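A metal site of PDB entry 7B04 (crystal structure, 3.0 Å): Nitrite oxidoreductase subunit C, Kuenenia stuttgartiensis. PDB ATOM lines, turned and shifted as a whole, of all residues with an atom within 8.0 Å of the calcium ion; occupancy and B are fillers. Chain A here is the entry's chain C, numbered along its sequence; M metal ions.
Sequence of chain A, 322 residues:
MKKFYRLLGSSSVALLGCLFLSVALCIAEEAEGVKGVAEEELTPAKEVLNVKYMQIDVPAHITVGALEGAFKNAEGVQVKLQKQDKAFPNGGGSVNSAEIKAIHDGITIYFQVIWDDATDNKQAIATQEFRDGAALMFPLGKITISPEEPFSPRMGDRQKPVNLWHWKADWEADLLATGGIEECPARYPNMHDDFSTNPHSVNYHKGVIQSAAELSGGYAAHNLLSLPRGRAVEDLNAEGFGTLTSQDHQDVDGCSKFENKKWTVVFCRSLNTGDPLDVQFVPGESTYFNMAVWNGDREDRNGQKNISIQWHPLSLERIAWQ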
ATOM      1  N   SER A  94       3.787  -4.435  36.610  1.00  0.00           N
ATOM      2  CA  SER A  94       2.508  -4.339  35.931  1.00  0.00           C
ATOM      3  C   SER A  94       2.221  -5.554  35.069  1.00  0.00           C
ATOM      4  O   SER A  94       1.059  -5.919  34.874  1.00  0.00           O
ATOM      5  CB  SER A  94       2.476  -3.062  35.079  1.00  0.00           C
ATOM      6  OG  SER A  94       3.747  -2.785  34.535  1.00  0.00           O
ATOM      7  N   VAL A  95       3.259  -6.197  34.533  1.00  0.00           N
ATOM      8  CA  VAL A  95       3.117  -7.385  33.717  1.00  0.00           C
ATOM      9  C   VAL A  95       3.826  -8.544  34.417  1.00  0.00           C
ATOM     10  O   VAL A  95       4.940  -8.380  34.921  1.00  0.00           O
ATOM     11  CB  VAL A  95       3.706  -7.168  32.308  1.00  0.00           C
ATOM     12  CG1 VAL A  95       3.595  -8.442  31.476  1.00  0.00           C
ATOM     13  CG2 VAL A  95       3.007  -6.007  31.608  1.00  0.00           C
ATOM     14  N   TRP A 115       2.074 -10.322  25.638  1.00  0.00           N
ATOM     15  CA  TRP A 115       1.778 -10.062  27.035  1.00  0.00           C
ATOM     16  C   TRP A 115       0.516  -9.211  27.096  1.00  0.00           C
ATOM     17  O   TRP A 115       0.122  -8.579  26.113  1.00  0.00           O
ATOM     18  CB  TRP A 115       2.935  -9.351  27.744  1.00  0.00           C
ATOM     19  CG  TRP A 115       3.130  -7.926  27.321  1.00  0.00           C
ATOM     20  CD1 TRP A 115       2.670  -6.816  27.954  1.00  0.00           C
ATOM     21  CD2 TRP A 115       3.841  -7.475  26.166  1.00  0.00           C
ATOM     22  NE1 TRP A 115       3.055  -5.686  27.266  1.00  0.00           N
ATOM     23  CE2 TRP A 115       3.777  -6.061  26.165  1.00  0.00           C
ATOM     24  CE3 TRP A 115       4.539  -8.122  25.137  1.00  0.00           C
ATOM     25  CZ2 TRP A 115       4.378  -5.294  25.171  1.00  0.00           C
ATOM     26  CZ3 TRP A 115       5.129  -7.352  24.156  1.00  0.00           C
ATOM     27  CH2 TRP A 115       5.037  -5.952  24.173  1.00  0.00           C
ATOM     28  N   ASP A 116      -0.122  -9.213  28.261  1.00  0.00           N
ATOM     29  CA  ASP A 116      -1.378  -8.504  28.447  1.00  0.00           C
ATOM     30  C   ASP A 116      -1.145  -7.143  29.069  1.00  0.00           C
ATOM     31  O   ASP A 116      -0.463  -7.015  30.083  1.00  0.00           O
ATOM     32  CB  ASP A 116      -2.353  -9.280  29.329  1.00  0.00           C
ATOM     33  CG  ASP A 116      -2.458 -10.744  28.938  1.00  0.00           C
ATOM     34  OD1 ASP A 116      -2.952 -11.007  27.824  1.00  0.00           O
ATOM     35  OD2 ASP A 116      -2.085 -11.617  29.744  1.00  0.00           O
ATOM     36  N   ASP A 117      -1.643  -6.109  28.413  1.00  0.00           N
ATOM     37  CA  ASP A 117      -1.578  -4.773  29.002  1.00  0.00           C
ATOM     38  C   ASP A 117      -2.756  -3.934  28.543  1.00  0.00           C
ATOM     39  O   ASP A 117      -3.131  -3.944  27.377  1.00  0.00           O
ATOM     40  CB  ASP A 117      -0.192  -4.112  28.820  1.00  0.00           C
ATOM     41  CG  ASP A 117      -0.217  -2.571  28.935  1.00  0.00           C
ATOM     42  OD1 ASP A 117      -0.424  -2.074  30.068  1.00  0.00           O
ATOM     43  OD2 ASP A 117       0.251  -1.933  27.906  1.00  0.00           O
ATOM     44  N   ALA A 118      -3.406  -3.312  29.526  1.00  0.00           N
ATOM     45  CA  ALA A 118      -4.691  -2.641  29.371  1.00  0.00           C
ATOM     46  C   ALA A 118      -4.598  -1.272  28.713  1.00  0.00           C
ATOM     47  O   ALA A 118      -5.640  -0.696  28.396  1.00  0.00           O
ATOM     48  CB  ALA A 118      -5.351  -2.492  30.742  1.00  0.00           C
ATOM     49  N   THR A 119      -3.391  -0.761  28.467  1.00  0.00           N
ATOM     50  CA  THR A 119      -3.220   0.600  27.974  1.00  0.00           C
ATOM     51  C   THR A 119      -2.310   0.590  26.756  1.00  0.00           C
ATOM     52  O   THR A 119      -1.300  -0.103  26.732  1.00  0.00           O
ATOM     53  CB  THR A 119      -2.638   1.523  29.056  1.00  0.00           C
ATOM     54  OG1 THR A 119      -1.300   1.136  29.359  1.00  0.00           O
ATOM     55  CG2 THR A 119      -3.487   1.481  30.325  1.00  0.00           C
ATOM     56  N   ASP A 120      -2.707   1.376  25.751  1.00  0.00           N
ATOM     57  CA  ASP A 120      -1.898   1.579  24.551  1.00  0.00           C
ATOM     58  C   ASP A 120      -1.135   2.895  24.701  1.00  0.00           C
ATOM     59  O   ASP A 120      -1.633   3.969  24.366  1.00  0.00           O
ATOM     60  CB  ASP A 120      -2.802   1.606  23.312  1.00  0.00           C
ATOM     61  CG  ASP A 120      -4.095   2.384  23.550  1.00  0.00           C
ATOM     62  OD1 ASP A 120      -4.489   3.179  22.679  1.00  0.00           O
ATOM     63  OD2 ASP A 120      -4.718   2.191  24.624  1.00  0.00           O
ATOM     64  N   ASN A 121       0.099   2.800  25.198  1.00  0.00           N
ATOM     65  CA  ASN A 121       0.994   3.953  25.282  1.00  0.00           C
ATOM     66  C   ASN A 121       1.868   3.924  24.036  1.00  0.00           C
ATOM     67  O   ASN A 121       2.818   3.144  23.947  1.00  0.00           O
ATOM     68  CB  ASN A 121       1.825   3.925  26.558  1.00  0.00           C
ATOM     69  CG  ASN A 121       0.968   3.830  27.817  1.00  0.00           C
ATOM     70  OD1 ASN A 121       1.070   2.854  28.553  1.00  0.00           O
ATOM     71  ND2 ASN A 121       0.145   4.842  28.061  1.00  0.00           N
ATOM     72  N   LYS A 122       1.541   4.759  23.059  1.00  0.00           N
ATOM     73  CA  LYS A 122       2.173   4.722  21.747  1.00  0.00           C
ATOM     74  C   LYS A 122       3.003   5.953  21.433  1.00  0.00           C
ATOM     75  O   LYS A 122       3.346   6.173  20.268  1.00  0.00           O
ATOM     76  CB  LYS A 122       1.105   4.540  20.668  1.00  0.00           C
ATOM     77  CG  LYS A 122       0.399   3.206  20.746  1.00  0.00           C
ATOM     78  CD  LYS A 122      -0.651   3.087  19.660  1.00  0.00           C
ATOM     79  CE  LYS A 122      -1.359   1.755  19.761  1.00  0.00           C
ATOM     80  NZ  LYS A 122      -2.395   1.613  18.708  1.00  0.00           N
ATOM     81  N   PHE A 130       5.187   7.999  28.833  1.00  0.00           N
ATOM     82  CA  PHE A 130       6.225   7.059  28.466  1.00  0.00           C
ATOM     83  C   PHE A 130       5.653   6.024  27.521  1.00  0.00           C
ATOM     84  O   PHE A 130       4.439   5.887  27.361  1.00  0.00           O
ATOM     85  CB  PHE A 130       6.816   6.370  29.717  1.00  0.00           C
ATOM     86  CG  PHE A 130       7.383   7.326  30.715  1.00  0.00           C
ATOM     87  CD1 PHE A 130       8.740   7.631  30.721  1.00  0.00           C
ATOM     88  CD2 PHE A 130       6.575   7.928  31.655  1.00  0.00           C
ATOM     89  CE1 PHE A 130       9.264   8.513  31.659  1.00  0.00           C
ATOM     90  CE2 PHE A 130       7.100   8.811  32.593  1.00  0.00           C
ATOM     91  CZ  PHE A 130       8.441   9.093  32.590  1.00  0.00           C
ATOM     92  N   ARG A 131       6.541   5.241  26.914  1.00  0.00           N
ATOM     93  CA  ARG A 131       6.151   4.326  25.868  1.00  0.00           C
ATOM     94  C   ARG A 131       6.061   2.914  26.422  1.00  0.00           C
ATOM     95  O   ARG A 131       6.811   2.536  27.327  1.00  0.00           O
ATOM     96  CB  ARG A 131       7.144   4.348  24.701  1.00  0.00           C
ATOM     97  CG  ARG A 131       8.539   3.957  25.174  1.00  0.00           C
ATOM     98  CD  ARG A 131       9.471   3.658  24.017  1.00  0.00           C
ATOM     99  NE  ARG A 131       9.986   4.878  23.424  1.00  0.00           N
ATOM    100  CZ  ARG A 131      11.098   5.471  23.837  1.00  0.00           C
ATOM    101  NH1 ARG A 131      11.802   4.961  24.842  1.00  0.00           N
ATOM    102  NH2 ARG A 131      11.504   6.584  23.248  1.00  0.00           N
ATOM    103  N   ASP A 132       5.176   2.121  25.825  1.00  0.00           N
ATOM    104  CA  ASP A 132       5.207   0.682  26.044  1.00  0.00           C
ATOM    105  C   ASP A 132       6.310   0.074  25.205  1.00  0.00           C
ATOM    106  O   ASP A 132       6.493   0.452  24.049  1.00  0.00           O
ATOM    107  CB  ASP A 132       3.879   0.031  25.718  1.00  0.00           C
ATOM    108  CG  ASP A 132       2.844   0.256  26.784  1.00  0.00           C
ATOM    109  OD1 ASP A 132       1.872   0.965  26.508  1.00  0.00           O
ATOM    110  OD2 ASP A 132       3.021  -0.259  27.916  1.00  0.00           O
ATOM    111  N   GLY A 133       7.043  -0.858  25.781  1.00  0.00           N
ATOM    112  CA  GLY A 133       8.162  -1.466  25.081  1.00  0.00           C
ATOM    113  C   GLY A 133       8.381  -2.906  25.485  1.00  0.00           C
ATOM    114  O   GLY A 133       7.904  -3.371  26.523  1.00  0.00           O
ATOM    115  N   ALA A 169       7.010   1.148  21.086  1.00  0.00           N
ATOM    116  CA  ALA A 169       5.678   1.364  20.537  1.00  0.00           C
ATOM    117  C   ALA A 169       5.597   2.702  19.800  1.00  0.00           C
ATOM    118  O   ALA A 169       4.915   2.803  18.774  1.00  0.00           O
ATOM    119  CB  ALA A 169       4.628   1.289  21.641  1.00  0.00           C
ATOM    120  N   PHE A 258      -1.673  -4.091  18.901  1.00  0.00           N
ATOM    121  CA  PHE A 258      -2.342  -4.022  20.196  1.00  0.00           C
ATOM    122  C   PHE A 258      -3.842  -4.165  19.995  1.00  0.00           C
ATOM    123  O   PHE A 258      -4.457  -3.332  19.326  1.00  0.00           O
ATOM    124  CB  PHE A 258      -2.032  -2.706  20.915  1.00  0.00           C
ATOM    125  CG  PHE A 258      -2.736  -2.579  22.236  1.00  0.00           C
ATOM    126  CD1 PHE A 258      -2.234  -3.214  23.363  1.00  0.00           C
ATOM    127  CD2 PHE A 258      -3.895  -1.830  22.357  1.00  0.00           C
ATOM    128  CE1 PHE A 258      -2.879  -3.104  24.576  1.00  0.00           C
ATOM    129  CE2 PHE A 258      -4.540  -1.723  23.579  1.00  0.00           C
ATOM    130  CZ  PHE A 258      -4.039  -2.351  24.688  1.00  0.00           C
ATOM    131  N   TRP A 263      -0.822  -6.936  23.827  1.00  0.00           N
ATOM    132  CA  TRP A 263       0.217  -6.606  22.852  1.00  0.00           C
ATOM    133  C   TRP A 263       0.706  -7.882  22.180  1.00  0.00           C
ATOM    134  O   TRP A 263       0.875  -8.917  22.832  1.00  0.00           O
ATOM    135  CB  TRP A 263       1.397  -5.899  23.504  1.00  0.00           C
ATOM    136  CG  TRP A 263       1.239  -4.414  23.647  1.00  0.00           C
ATOM    137  CD1 TRP A 263       0.991  -3.732  24.795  1.00  0.00           C
ATOM    138  CD2 TRP A 263       1.324  -3.436  22.598  1.00  0.00           C
ATOM    139  NE1 TRP A 263       0.911  -2.385  24.528  1.00  0.00           N
ATOM    140  CE2 TRP A 263       1.119  -2.179  23.191  1.00  0.00           C
ATOM    141  CE3 TRP A 263       1.556  -3.507  21.219  1.00  0.00           C
ATOM    142  CZ2 TRP A 263       1.125  -0.996  22.449  1.00  0.00           C
ATOM    143  CZ3 TRP A 263       1.574  -2.339  20.491  1.00  0.00           C
ATOM    144  CH2 TRP A 263       1.361  -1.096  21.112  1.00  0.00           C
ATOM    145  N   TRP A 294       8.011  -3.293  29.210  1.00  0.00           N
ATOM    146  CA  TRP A 294       7.758  -2.008  29.840  1.00  0.00           C
ATOM    147  C   TRP A 294       6.309  -1.603  29.638  1.00  0.00           C
ATOM    148  O   TRP A 294       5.705  -1.894  28.606  1.00  0.00           O
ATOM    149  CB  TRP A 294       8.680  -0.915  29.279  1.00  0.00           C
ATOM    150  CG  TRP A 294      10.123  -1.170  29.567  1.00  0.00           C
ATOM    151  CD1 TRP A 294      10.875  -0.627  30.565  1.00  0.00           C
ATOM    152  CD2 TRP A 294      10.980  -2.072  28.856  1.00  0.00           C
ATOM    153  NE1 TRP A 294      12.149  -1.121  30.512  1.00  0.00           N
ATOM    154  CE2 TRP A 294      12.236  -2.011  29.472  1.00  0.00           C
ATOM    155  CE3 TRP A 294      10.801  -2.914  27.764  1.00  0.00           C
ATOM    156  CZ2 TRP A 294      13.325  -2.760  29.029  1.00  0.00           C
ATOM    157  CZ3 TRP A 294      11.869  -3.655  27.315  1.00  0.00           C
ATOM    158  CH2 TRP A 294      13.111  -3.583  27.947  1.00  0.00           C
ATOM    159  N   ASN A 295       5.755  -0.908  30.635  1.00  0.00           N
ATOM    160  CA  ASN A 295       4.403  -0.362  30.551  1.00  0.00           C
ATOM    161  C   ASN A 295       4.454   1.126  30.857  1.00  0.00           C
ATOM    162  O   ASN A 295       4.650   1.521  32.011  1.00  0.00           O
ATOM    163  CB  ASN A 295       3.452  -1.077  31.511  1.00  0.00           C
ATOM    164  CG  ASN A 295       1.997  -0.688  31.292  1.00  0.00           C
ATOM    165  OD1 ASN A 295       1.642  -0.090  30.282  1.00  0.00           O
ATOM    166  ND2 ASN A 295       1.151  -1.011  32.259  1.00  0.00           N
ATOM    167  N   GLY A 296       4.286   1.951  29.812  1.00  0.00           N
ATOM    168  CA  GLY A 296       4.312   3.392  29.981  1.00  0.00           C
ATOM    169  C   GLY A 296       3.264   3.918  30.935  1.00  0.00           C
ATOM    170  O   GLY A 296       3.439   5.000  31.499  1.00  0.00           O
ATOM    171  N   ASP A 297       2.173   3.176  31.133  1.00  0.00           N
ATOM    172  CA  ASP A 297       1.132   3.633  32.047  1.00  0.00           C
ATOM    173  C   ASP A 297       1.649   3.697  33.477  1.00  0.00           C
ATOM    174  O   ASP A 297       1.264   4.589  34.243  1.00  0.00           O
ATOM    175  CB  ASP A 297      -0.093   2.718  31.951  1.00  0.00           C
ATOM    176  CG  ASP A 297      -1.307   3.295  32.643  1.00  0.00           C
ATOM    177  OD1 ASP A 297      -1.902   4.246  32.099  1.00  0.00           O
ATOM    178  OD2 ASP A 297      -1.677   2.802  33.728  1.00  0.00           O
ATOM    179  N   ARG A 298       2.515   2.755  33.868  1.00  0.00           N
ATOM    180  CA  ARG A 298       3.170   2.776  35.164  1.00  0.00           C
ATOM    181  C   ARG A 298       4.566   3.417  35.113  1.00  0.00           C
ATOM    182  O   ARG A 298       5.376   3.180  36.010  1.00  0.00           O
ATOM    183  CB  ARG A 298       3.265   1.357  35.736  1.00  0.00           C
ATOM    184  CG  ARG A 298       1.968   0.865  36.376  1.00  0.00           C
ATOM    185  CD  ARG A 298       1.111   0.150  35.354  1.00  0.00           C
ATOM    186  NE  ARG A 298       0.103  -0.710  35.975  1.00  0.00           N
ATOM    187  CZ  ARG A 298      -1.181  -0.400  36.060  1.00  0.00           C
ATOM    188  NH1 ARG A 298      -1.619   0.751  35.580  1.00  0.00           N
ATOM    189  NH2 ARG A 298      -2.026  -1.249  36.643  1.00  0.00           N
HETATM  190 CA    CA M   1       0.519   0.316  28.226  1.00  0.00          CA
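OD2 of Asp 132 sits close to N of Gly 296. The side-chain amide oxygen of Asn 295 lies close to the backbone NH of Asp 297, at 3.4 Å. The backbone NH (N) of Ala 169 lies within hydrogen-bond range of the backbone carbonyl oxygen (O) of Asp 132 (3.1 Å). The side-chain amide oxygen (OD1) of Asn 121 sits close to the backbone NH (N) of Asp 297 (2.8 Å). The side-chain carboxylate of Asp 117 lies close to the indole nitrogen of Trp 263 (3.5 Å).
Five residues have an atom within 4 Å of the calcium ion: Asp 117, Thr 119, Asn 121, Asp 132 and Asn 295. The nearest printed residue that does not touch the calcium ion is Asp 120 (4.2 Å).
OD1 of Asp 132 binds the calcium ion. OD2 of Asp 117 is bound to the calcium ion (2.3 Å). The side-chain hydroxyl (OG1) of Thr 119 is bound to the calcium ion, at 2.3 Å. The side-chain amide oxygen (OD1) of Asn 295 binds the calcium ion. The calcium ion is bound by O of Thr 119 (2.4 Å). The side-chain carboxylate (OD2) of Asp 132 binds the calcium ion. The side-chain amide oxygen (OD1) of Asn 121 is bound to the calcium ion, at 2.6 Å. The calcium ion has seven donor atoms within binding distance.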
